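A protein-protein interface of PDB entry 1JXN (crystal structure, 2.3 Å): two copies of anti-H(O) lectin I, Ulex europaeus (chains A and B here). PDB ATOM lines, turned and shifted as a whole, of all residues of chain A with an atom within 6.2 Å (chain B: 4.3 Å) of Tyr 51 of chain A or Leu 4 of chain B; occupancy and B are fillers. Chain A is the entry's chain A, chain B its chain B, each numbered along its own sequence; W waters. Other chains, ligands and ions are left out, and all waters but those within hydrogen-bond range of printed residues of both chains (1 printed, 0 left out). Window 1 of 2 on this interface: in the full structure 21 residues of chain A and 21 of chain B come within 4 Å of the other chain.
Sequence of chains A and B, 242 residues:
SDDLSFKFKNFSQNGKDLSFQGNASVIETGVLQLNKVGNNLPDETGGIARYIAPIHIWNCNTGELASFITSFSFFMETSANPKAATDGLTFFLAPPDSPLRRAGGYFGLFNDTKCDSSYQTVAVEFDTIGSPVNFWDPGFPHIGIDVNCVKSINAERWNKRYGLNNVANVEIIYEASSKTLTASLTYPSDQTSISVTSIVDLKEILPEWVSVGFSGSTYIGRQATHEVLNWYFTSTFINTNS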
ATOM      1  N   LEU A   4     -15.094  -6.188   0.336  1.00  0.00           N
ATOM      2  CA  LEU A   4     -14.348  -7.416   0.146  1.00  0.00           C
ATOM      3  C   LEU A   4     -14.594  -7.874  -1.272  1.00  0.00           C
ATOM      4  O   LEU A   4     -15.641  -7.587  -1.857  1.00  0.00           O
ATOM      5  CB  LEU A   4     -14.812  -8.493   1.129  1.00  0.00           C
ATOM      6  CG  LEU A   4     -13.869  -9.639   1.530  1.00  0.00           C
ATOM      7  CD1 LEU A   4     -14.642 -10.924   1.528  1.00  0.00           C
ATOM      8  CD2 LEU A   4     -12.664  -9.786   0.620  1.00  0.00           C
ATOM      9  N   SER A   5     -13.581  -8.481  -1.860  1.00  0.00           N
ATOM     10  CA  SER A   5     -13.685  -8.995  -3.205  1.00  0.00           C
ATOM     11  C   SER A   5     -12.514  -9.909  -3.449  1.00  0.00           C
ATOM     12  O   SER A   5     -11.398  -9.662  -2.996  1.00  0.00           O
ATOM     13  CB  SER A   5     -13.726  -7.859  -4.234  1.00  0.00           C
ATOM     14  OG  SER A   5     -12.842  -6.807  -3.894  1.00  0.00           O
ATOM     15  N   PHE A   6     -12.795 -11.011  -4.105  1.00  0.00           N
ATOM     16  CA  PHE A   6     -11.770 -11.974  -4.413  1.00  0.00           C
ATOM     17  C   PHE A   6     -12.224 -12.700  -5.653  1.00  0.00           C
ATOM     18  O   PHE A   6     -13.420 -12.966  -5.842  1.00  0.00           O
ATOM     19  CB  PHE A   6     -11.578 -12.944  -3.248  1.00  0.00           C
ATOM     20  CG  PHE A   6     -12.852 -13.619  -2.785  1.00  0.00           C
ATOM     21  CD1 PHE A   6     -13.383 -14.713  -3.480  1.00  0.00           C
ATOM     22  CD2 PHE A   6     -13.509 -13.180  -1.638  1.00  0.00           C
ATOM     23  CE1 PHE A   6     -14.530 -15.346  -3.039  1.00  0.00           C
ATOM     24  CE2 PHE A   6     -14.666 -13.822  -1.194  1.00  0.00           C
ATOM     25  CZ  PHE A   6     -15.171 -14.906  -1.901  1.00  0.00           C
ATOM     26  N   LYS A   7     -11.281 -13.003  -6.522  1.00  0.00           N
ATOM     27  CA  LYS A   7     -11.632 -13.690  -7.732  1.00  0.00           C
ATOM     28  C   LYS A   7     -10.740 -14.876  -7.862  1.00  0.00           C
ATOM     29  O   LYS A   7      -9.551 -14.780  -7.601  1.00  0.00           O
ATOM     30  CB  LYS A   7     -11.450 -12.779  -8.945  1.00  0.00           C
ATOM     31  CG  LYS A   7     -11.753 -13.487 -10.247  1.00  0.00           C
ATOM     32  CD  LYS A   7     -12.316 -12.549 -11.286  1.00  0.00           C
ATOM     33  CE  LYS A   7     -11.233 -11.767 -11.983  1.00  0.00           C
ATOM     34  NZ  LYS A   7     -11.835 -10.774 -12.910  1.00  0.00           N
ATOM     35  N   PHE A   8     -11.340 -16.011  -8.184  1.00  0.00           N
ATOM     36  CA  PHE A   8     -10.615 -17.249  -8.405  1.00  0.00           C
ATOM     37  C   PHE A   8     -10.852 -17.532  -9.890  1.00  0.00           C
ATOM     38  O   PHE A   8     -11.993 -17.680 -10.322  1.00  0.00           O
ATOM     39  CB  PHE A   8     -11.205 -18.411  -7.604  1.00  0.00           C
ATOM     40  CG  PHE A   8     -10.993 -18.336  -6.113  1.00  0.00           C
ATOM     41  CD1 PHE A   8     -10.087 -19.191  -5.488  1.00  0.00           C
ATOM     42  CD2 PHE A   8     -11.781 -17.502  -5.320  1.00  0.00           C
ATOM     43  CE1 PHE A   8      -9.983 -19.226  -4.104  1.00  0.00           C
ATOM     44  CE2 PHE A   8     -11.685 -17.526  -3.935  1.00  0.00           C
ATOM     45  CZ  PHE A   8     -10.790 -18.388  -3.322  1.00  0.00           C
ATOM     46  N   ASP A  17      -7.129 -20.784   1.289  1.00  0.00           N
ATOM     47  CA  ASP A  17      -8.233 -19.890   1.611  1.00  0.00           C
ATOM     48  C   ASP A  17      -9.647 -20.479   1.400  1.00  0.00           C
ATOM     49  O   ASP A  17     -10.606 -19.742   1.153  1.00  0.00           O
ATOM     50  CB  ASP A  17      -8.075 -18.557   0.879  1.00  0.00           C
ATOM     51  CG  ASP A  17      -8.078 -18.698  -0.631  1.00  0.00           C
ATOM     52  OD1 ASP A  17      -7.968 -17.656  -1.311  1.00  0.00           O
ATOM     53  OD2 ASP A  17      -8.183 -19.826  -1.149  1.00  0.00           O
ATOM     54  N   LEU A  18      -9.776 -21.799   1.538  1.00  0.00           N
ATOM     55  CA  LEU A  18     -11.065 -22.486   1.381  1.00  0.00           C
ATOM     56  C   LEU A  18     -11.203 -23.636   2.364  1.00  0.00           C
ATOM     57  O   LEU A  18     -10.327 -24.487   2.451  1.00  0.00           O
ATOM     58  CB  LEU A  18     -11.228 -23.070  -0.028  1.00  0.00           C
ATOM     59  CG  LEU A  18     -11.474 -22.242  -1.287  1.00  0.00           C
ATOM     60  CD1 LEU A  18     -11.610 -23.207  -2.445  1.00  0.00           C
ATOM     61  CD2 LEU A  18     -12.723 -21.375  -1.178  1.00  0.00           C
ATOM     62  N   SER A  19     -12.303 -23.675   3.103  1.00  0.00           N
ATOM     63  CA  SER A  19     -12.532 -24.771   4.035  1.00  0.00           C
ATOM     64  C   SER A  19     -13.551 -25.696   3.392  1.00  0.00           C
ATOM     65  O   SER A  19     -14.549 -25.243   2.831  1.00  0.00           O
ATOM     66  CB  SER A  19     -13.030 -24.267   5.386  1.00  0.00           C
ATOM     67  OG  SER A  19     -14.176 -23.465   5.234  1.00  0.00           O
ATOM     68  N   ALA A  49     -17.878 -25.982   0.377  1.00  0.00           N
ATOM     69  CA  ALA A  49     -16.590 -25.319   0.204  1.00  0.00           C
ATOM     70  C   ALA A  49     -16.857 -23.828   0.350  1.00  0.00           C
ATOM     71  O   ALA A  49     -17.526 -23.236  -0.494  1.00  0.00           O
ATOM     72  CB  ALA A  49     -15.994 -25.632  -1.179  1.00  0.00           C
ATOM     73  N   ARG A  50     -16.353 -23.223   1.420  1.00  0.00           N
ATOM     74  CA  ARG A  50     -16.592 -21.795   1.639  1.00  0.00           C
ATOM     75  C   ARG A  50     -15.327 -20.964   1.783  1.00  0.00           C
ATOM     76  O   ARG A  50     -14.274 -21.505   2.110  1.00  0.00           O
ATOM     77  CB  ARG A  50     -17.498 -21.590   2.862  1.00  0.00           C
ATOM     78  CG  ARG A  50     -17.125 -22.445   4.049  1.00  0.00           C
ATOM     79  CD  ARG A  50     -18.138 -22.316   5.178  1.00  0.00           C
ATOM     80  NE  ARG A  50     -18.959 -23.511   5.360  1.00  0.00           N
ATOM     81  CZ  ARG A  50     -20.059 -23.543   6.108  1.00  0.00           C
ATOM     82  NH1 ARG A  50     -20.468 -22.448   6.738  1.00  0.00           N
ATOM     83  NH2 ARG A  50     -20.749 -24.666   6.238  1.00  0.00           N
ATOM     84  N   TYR A  51     -15.420 -19.663   1.506  1.00  0.00           N
ATOM     85  CA  TYR A  51     -14.264 -18.793   1.648  1.00  0.00           C
ATOM     86  C   TYR A  51     -13.872 -18.822   3.123  1.00  0.00           C
ATOM     87  O   TYR A  51     -14.727 -18.748   4.021  1.00  0.00           O
ATOM     88  CB  TYR A  51     -14.542 -17.368   1.178  1.00  0.00           C
ATOM     89  CG  TYR A  51     -13.287 -16.531   1.113  1.00  0.00           C
ATOM     90  CD1 TYR A  51     -13.120 -15.417   1.932  1.00  0.00           C
ATOM     91  CD2 TYR A  51     -12.235 -16.887   0.263  1.00  0.00           C
ATOM     92  CE1 TYR A  51     -11.928 -14.680   1.916  1.00  0.00           C
ATOM     93  CE2 TYR A  51     -11.036 -16.161   0.228  1.00  0.00           C
ATOM     94  CZ  TYR A  51     -10.889 -15.065   1.063  1.00  0.00           C
ATOM     95  OH  TYR A  51      -9.688 -14.387   1.086  1.00  0.00           O
ATOM     96  N   ILE A  52     -12.573 -19.005   3.351  1.00  0.00           N
ATOM     97  CA  ILE A  52     -11.995 -19.130   4.686  1.00  0.00           C
ATOM     98  C   ILE A  52     -12.301 -17.978   5.648  1.00  0.00           C
ATOM     99  O   ILE A  52     -12.452 -18.188   6.842  1.00  0.00           O
ATOM    100  CB  ILE A  52     -10.472 -19.375   4.587  1.00  0.00           C
ATOM    101  CG1 ILE A  52      -9.979 -20.196   5.766  1.00  0.00           C
ATOM    102  CG2 ILE A  52      -9.734 -18.069   4.496  1.00  0.00           C
ATOM    103  CD1 ILE A  52     -10.345 -21.639   5.675  1.00  0.00           C
ATOM    104  N   ALA A  53     -12.433 -16.774   5.128  1.00  0.00           N
ATOM    105  CA  ALA A  53     -12.725 -15.634   5.977  1.00  0.00           C
ATOM    106  C   ALA A  53     -14.205 -15.278   5.962  1.00  0.00           C
ATOM    107  O   ALA A  53     -14.835 -15.219   4.904  1.00  0.00           O
ATOM    108  CB  ALA A  53     -11.912 -14.431   5.535  1.00  0.00           C
ATOM    109  N   PRO A  54     -14.781 -15.069   7.151  1.00  0.00           N
ATOM    110  CA  PRO A  54     -16.189 -14.703   7.321  1.00  0.00           C
ATOM    111  C   PRO A  54     -16.416 -13.276   6.835  1.00  0.00           C
ATOM    112  O   PRO A  54     -15.587 -12.395   7.077  1.00  0.00           O
ATOM    113  CB  PRO A  54     -16.378 -14.805   8.832  1.00  0.00           C
ATOM    114  CG  PRO A  54     -15.407 -15.879   9.214  1.00  0.00           C
ATOM    115  CD  PRO A  54     -14.192 -15.492   8.428  1.00  0.00           C
ATOM    116  N   ILE A  55     -17.523 -13.075   6.116  1.00  0.00           N
ATOM    117  CA  ILE A  55     -17.932 -11.776   5.549  1.00  0.00           C
ATOM    118  C   ILE A  55     -18.738 -10.958   6.557  1.00  0.00           C
ATOM    119  O   ILE A  55     -19.579 -11.507   7.267  1.00  0.00           O
ATOM    120  CB  ILE A  55     -18.873 -11.968   4.326  1.00  0.00           C
ATOM    121  CG1 ILE A  55     -18.364 -13.078   3.405  1.00  0.00           C
ATOM    122  CG2 ILE A  55     -19.037 -10.650   3.564  1.00  0.00           C
ATOM    123  CD1 ILE A  55     -17.124 -12.741   2.630  1.00  0.00           C
ATOM    124  N   SER A 211     -20.466 -16.864   6.242  1.00  0.00           N
ATOM    125  CA  SER A 211     -19.568 -17.429   5.271  1.00  0.00           C
ATOM    126  C   SER A 211     -20.306 -17.402   3.941  1.00  0.00           C
ATOM    127  O   SER A 211     -21.523 -17.259   3.900  1.00  0.00           O
ATOM    128  CB  SER A 211     -19.154 -18.853   5.675  1.00  0.00           C
ATOM    129  OG  SER A 211     -20.254 -19.713   5.926  1.00  0.00           O
ATOM    130  N   VAL A 212     -19.553 -17.352   2.862  1.00  0.00           N
ATOM    131  CA  VAL A 212     -20.141 -17.366   1.542  1.00  0.00           C
ATOM    132  C   VAL A 212     -19.411 -18.518   0.874  1.00  0.00           C
ATOM    133  O   VAL A 212     -18.190 -18.659   1.043  1.00  0.00           O
ATOM    134  CB  VAL A 212     -19.918 -16.045   0.775  1.00  0.00           C
ATOM    135  CG1 VAL A 212     -20.565 -14.892   1.521  1.00  0.00           C
ATOM    136  CG2 VAL A 212     -18.433 -15.792   0.521  1.00  0.00           C
ATOM    137  N   GLY A 213     -20.152 -19.377   0.184  1.00  0.00           N
ATOM    138  CA  GLY A 213     -19.522 -20.504  -0.461  1.00  0.00           C
ATOM    139  C   GLY A 213     -20.464 -21.309  -1.301  1.00  0.00           C
ATOM    140  O   GLY A 213     -21.465 -20.798  -1.768  1.00  0.00           O
ATOM    141  N   TRP A 231     -14.883 -18.216  -9.674  1.00  0.00           N
ATOM    142  CA  TRP A 231     -15.724 -17.527  -8.700  1.00  0.00           C
ATOM    143  C   TRP A 231     -15.301 -16.080  -8.503  1.00  0.00           C
ATOM    144  O   TRP A 231     -14.115 -15.744  -8.529  1.00  0.00           O
ATOM    145  CB  TRP A 231     -15.669 -18.269  -7.358  1.00  0.00           C
ATOM    146  CG  TRP A 231     -16.571 -17.736  -6.253  1.00  0.00           C
ATOM    147  CD1 TRP A 231     -17.614 -16.856  -6.383  1.00  0.00           C
ATOM    148  CD2 TRP A 231     -16.539 -18.121  -4.865  1.00  0.00           C
ATOM    149  NE1 TRP A 231     -18.235 -16.680  -5.171  1.00  0.00           N
ATOM    150  CE2 TRP A 231     -17.602 -17.442  -4.223  1.00  0.00           C
ATOM    151  CE3 TRP A 231     -15.724 -18.978  -4.106  1.00  0.00           C
ATOM    152  CZ2 TRP A 231     -17.868 -17.593  -2.858  1.00  0.00           C
ATOM    153  CZ3 TRP A 231     -15.987 -19.133  -2.756  1.00  0.00           C
ATOM    154  CH2 TRP A 231     -17.052 -18.443  -2.143  1.00  0.00           C
ATOM    155  N   SER B   1      -6.822 -17.078  -3.678  1.00  0.00           N
ATOM    156  CA  SER B   1      -7.564 -16.408  -4.781  1.00  0.00           C
ATOM    157  C   SER B   1      -6.573 -15.805  -5.766  1.00  0.00           C
ATOM    158  O   SER B   1      -5.365 -15.805  -5.520  1.00  0.00           O
ATOM    159  CB  SER B   1      -8.463 -15.312  -4.202  1.00  0.00           C
ATOM    160  OG  SER B   1      -7.723 -14.418  -3.383  1.00  0.00           O
ATOM    161  N   ASP B   3      -7.201 -12.598  -7.365  1.00  0.00           N
ATOM    162  CA  ASP B   3      -7.261 -11.182  -7.025  1.00  0.00           C
ATOM    163  C   ASP B   3      -7.935 -11.099  -5.672  1.00  0.00           C
ATOM    164  O   ASP B   3      -8.813 -11.910  -5.363  1.00  0.00           O
ATOM    165  CB  ASP B   3      -8.109 -10.418  -8.045  1.00  0.00           C
ATOM    166  CG  ASP B   3      -7.533 -10.447  -9.448  1.00  0.00           C
ATOM    167  OD1 ASP B   3      -7.594  -9.413 -10.138  1.00  0.00           O
ATOM    168  OD2 ASP B   3      -7.037 -11.510  -9.895  1.00  0.00           O
ATOM    169  N   LEU B   4      -7.535 -10.139  -4.854  1.00  0.00           N
ATOM    170  CA  LEU B   4      -8.143  -9.970  -3.548  1.00  0.00           C
ATOM    171  C   LEU B   4      -7.965  -8.554  -3.055  1.00  0.00           C
ATOM    172  O   LEU B   4      -6.986  -7.891  -3.381  1.00  0.00           O
ATOM    173  CB  LEU B   4      -7.566 -10.969  -2.532  1.00  0.00           C
ATOM    174  CG  LEU B   4      -8.173 -10.941  -1.120  1.00  0.00           C
ATOM    175  CD1 LEU B   4      -8.163 -12.323  -0.530  1.00  0.00           C
ATOM    176  CD2 LEU B   4      -7.424  -9.965  -0.214  1.00  0.00           C
ATOM    177  N   SER B   5      -8.976  -8.060  -2.356  1.00  0.00           N
ATOM    178  CA  SER B   5      -8.934  -6.729  -1.775  1.00  0.00           C
ATOM    179  C   SER B   5      -9.996  -6.607  -0.706  1.00  0.00           C
ATOM    180  O   SER B   5     -11.028  -7.283  -0.755  1.00  0.00           O
ATOM    181  CB  SER B   5      -9.098  -5.630  -2.832  1.00  0.00           C
ATOM    182  OG  SER B   5     -10.422  -5.538  -3.315  1.00  0.00           O
ATOM    183  N   PHE B   6      -9.671  -5.847   0.324  1.00  0.00           N
ATOM    184  CA  PHE B   6     -10.589  -5.602   1.410  1.00  0.00           C
ATOM    185  C   PHE B   6     -10.335  -4.215   1.917  1.00  0.00           C
ATOM    186  O   PHE B   6      -9.382  -3.559   1.504  1.00  0.00           O
ATOM    187  CB  PHE B   6     -10.465  -6.645   2.525  1.00  0.00           C
ATOM    188  CG  PHE B   6      -9.085  -6.787   3.112  1.00  0.00           C
ATOM    189  CD1 PHE B   6      -8.513  -5.763   3.862  1.00  0.00           C
ATOM    190  CD2 PHE B   6      -8.389  -7.976   2.977  1.00  0.00           C
ATOM    191  CE1 PHE B   6      -7.289  -5.927   4.473  1.00  0.00           C
ATOM    192  CE2 PHE B   6      -7.161  -8.151   3.584  1.00  0.00           C
ATOM    193  CZ  PHE B   6      -6.614  -7.122   4.334  1.00  0.00           C
ATOM    194  N   TYR B  51      -5.180 -10.600   8.624  1.00  0.00           N
ATOM    195  CA  TYR B  51      -6.461 -10.863   7.971  1.00  0.00           C
ATOM    196  C   TYR B  51      -6.556 -12.383   7.939  1.00  0.00           C
ATOM    197  O   TYR B  51      -5.720 -13.046   7.336  1.00  0.00           O
ATOM    198  CB  TYR B  51      -6.493 -10.309   6.556  1.00  0.00           C
ATOM    199  CG  TYR B  51      -7.822 -10.546   5.907  1.00  0.00           C
ATOM    200  CD1 TYR B  51      -7.956 -11.456   4.864  1.00  0.00           C
ATOM    201  CD2 TYR B  51      -8.960  -9.903   6.377  1.00  0.00           C
ATOM    202  CE1 TYR B  51      -9.216 -11.730   4.300  1.00  0.00           C
ATOM    203  CE2 TYR B  51     -10.218 -10.165   5.829  1.00  0.00           C
ATOM    204  CZ  TYR B  51     -10.338 -11.079   4.792  1.00  0.00           C
ATOM    205  OH  TYR B  51     -11.578 -11.354   4.258  1.00  0.00           O
ATOM    206  N   ALA B  53      -7.609 -14.600   6.311  1.00  0.00           N
ATOM    207  CA  ALA B  53      -7.424 -15.355   5.082  1.00  0.00           C
ATOM    208  C   ALA B  53      -6.059 -15.211   4.392  1.00  0.00           C
ATOM    209  O   ALA B  53      -5.623 -14.104   4.056  1.00  0.00           O
ATOM    210  CB  ALA B  53      -8.544 -15.036   4.099  1.00  0.00           C
ATOM    211  N   ILE B  55      -3.250 -15.047   1.689  1.00  0.00           N
ATOM    212  CA  ILE B  55      -3.229 -14.466   0.362  1.00  0.00           C
ATOM    213  C   ILE B  55      -2.312 -15.285  -0.545  1.00  0.00           C
ATOM    214  O   ILE B  55      -1.278 -15.798  -0.107  1.00  0.00           O
ATOM    215  CB  ILE B  55      -2.687 -13.026   0.403  1.00  0.00           C
ATOM    216  CG1 ILE B  55      -3.264 -12.264   1.606  1.00  0.00           C
ATOM    217  CG2 ILE B  55      -2.962 -12.323  -0.909  1.00  0.00           C
ATOM    218  CD1 ILE B  55      -4.769 -12.182   1.655  1.00  0.00           C
ATOM    219  N   PHE B 233      -6.418  -2.971   1.505  1.00  0.00           N
ATOM    220  CA  PHE B 233      -5.479  -3.945   0.977  1.00  0.00           C
ATOM    221  C   PHE B 233      -5.977  -4.635  -0.281  1.00  0.00           C
ATOM    222  O   PHE B 233      -7.012  -5.281  -0.275  1.00  0.00           O
ATOM    223  CB  PHE B 233      -5.142  -5.012   2.020  1.00  0.00           C
ATOM    224  CG  PHE B 233      -4.191  -6.068   1.508  1.00  0.00           C
ATOM    225  CD1 PHE B 233      -2.822  -5.939   1.698  1.00  0.00           C
ATOM    226  CD2 PHE B 233      -4.664  -7.157   0.776  1.00  0.00           C
ATOM    227  CE1 PHE B 233      -1.941  -6.867   1.168  1.00  0.00           C
ATOM    228  CE2 PHE B 233      -3.790  -8.088   0.243  1.00  0.00           C
ATOM    229  CZ  PHE B 233      -2.419  -7.942   0.437  1.00  0.00           C
ATOM    230  N   THR B 234      -5.192  -4.550  -1.340  1.00  0.00           N
ATOM    231  CA  THR B 234      -5.538  -5.191  -2.586  1.00  0.00           C
ATOM    232  C   THR B 234      -4.302  -5.857  -3.156  1.00  0.00           C
ATOM    233  O   THR B 234      -3.176  -5.421  -2.942  1.00  0.00           O
ATOM    234  CB  THR B 234      -6.111  -4.221  -3.621  1.00  0.00           C
ATOM    235  OG1 THR B 234      -6.373  -4.933  -4.835  1.00  0.00           O
ATOM    236  CG2 THR B 234      -5.142  -3.104  -3.915  1.00  0.00           C
ATOM    237  N   SER B 235      -4.532  -6.918  -3.900  1.00  0.00           N
ATOM    238  CA  SER B 235      -3.477  -7.682  -4.519  1.00  0.00           C
ATOM    239  C   SER B 235      -4.100  -8.373  -5.707  1.00  0.00           C
ATOM    240  O   SER B 235      -5.286  -8.738  -5.691  1.00  0.00           O
ATOM    241  CB  SER B 235      -2.956  -8.726  -3.542  1.00  0.00           C
ATOM    242  OG  SER B 235      -4.030  -9.442  -2.955  1.00  0.00           O
HETATM  243  O   HOH W   1      -7.294 -15.408  -0.178  1.00  0.00           O
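N of Lys 7 of chain A sits at hydrogen-bond distance from O of Asp 3 of chain B, 2.9 Å away. N of Ser 1 of chain B lies within hydrogen-bond range of OD1 of Asp 17 of chain A (2.7 Å). The side-chain hydroxyl of Ser 5 of chain B is in hydrogen-bond range of the side-chain hydroxyl of Ser 5 of chain A.
O of Asp 17 of chain A lies within hydrogen-bond range of N of Ile 52 of chain A, 3.0 Å away. O of Leu 4 of chain B sits at hydrogen-bond distance from N of Ser 235 of chain B, 2.7 Å away. The side-chain hydroxyl (OG) of Ser 1 of chain B sits at hydrogen-bond distance from the backbone carbonyl oxygen (O) of Asp 3 of chain B. The side-chain hydroxyl (OG1) of Thr 234 of chain B sits close to the backbone carbonyl oxygen (O) of Leu 4 of chain B (3.4 Å). The backbone carbonyl oxygen (O) of Val 212 of chain A sits at hydrogen-bond distance from the backbone NH (N) of Tyr 51 of chain A (3.0 Å). The backbone NH (N) of Phe 8 of chain A is in hydrogen-bond range of the backbone carbonyl oxygen (O) of Trp 231 of chain A, at 2.8 Å.
CD2 of Leu 4 of chain A touches O of Ser 5 of chain B (3.3 Å). Leu 4 of chain A touches Tyr 51 of chain B. O of Ser 5 of chain A touches CA of Leu 4 of chain B, at 3.3 Å. CA of Phe 6 of chain A touches O of Asp 3 of chain B (3.1 Å). Lys 7 of chain A touches Ser 1 of chain B. Phe 8 of chain A touches Ser 1 of chain B. Tyr 51 of chain A touches Ala 53 of chain B. CB of Ala 53 of chain B touches CG2 of Ile 52 of chain A, 3.3 Å away. OH of Tyr 51 of chain B touches CB of Ala 53 of chain A (3.3 Å). CB of Ala 53 of chain B touches CB of Ala 53 of chain A, at 3.7 Å.
Of the printed residues of chain B, Phe 8 of chain A touches Ser 1. Of chain B, only Leu 4 (3.0 Å) and Ala 53 (3.3 Å) come within 4 Å of Tyr 51 of chain A. Printed residues of chain B within 4 Å of Ile 52 of chain A: Ala 53. Trp 231 of chain A touches none of the printed residues of chain B. Leu 4 of chain B touches just these residues of chain A: Ser 5 (3.3 Å) and Tyr 51 (3.0 Å). Of the printed residues of chain A, Ser 5 of chain B touches Leu 4 (3.3 Å) and Ser 5 (2.8 Å). Printed residues of chain A within 4 Å of Ala 53 of chain B: Tyr 51 (3.3 Å), Ile 52 (3.3 Å) and Ala 53 (3.7 Å). The nearest residue of chain A that does not touch Leu 4 of chain B is Phe 6 of chain A (4.2 Å).
Hydrophobic or aromatic side chains of chain A that line the printed part of chain B: Leu 4, Phe 6, Phe 8, Tyr 51, Ile 52 and Ala 53. Hydrophobic or aromatic side chains of chain B that line the printed part of chain A: Leu 4, Tyr 51 and Ala 53.
Leu 4 of chain A touches Tyr 51 of chain B, and with the chains exchanged Tyr 51 of chain A touches Leu 4 of chain B. Ser 5 of chain B touches its own counterpart, Ser 5 of chain A. Tyr 51 of chain A touches Ala 53 of chain B, and with the chains exchanged Ala 53 of chain A touches Tyr 51 of chain B. Ala 53 of chain A touches its own counterpart, Ala 53 of chain B. Of the 14 pairs that touch across the chains among the printed residues, 8 have their exchanged pair printed and touching as well.
Water W1 lies within hydrogen-bond range of the side-chain carboxylate (OD1) of Asp 17 of chain A, the side-chain hydroxyl (OH) of Tyr 51 of chain A and the side-chain hydroxyl (OG) of Ser 1 of chain B.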
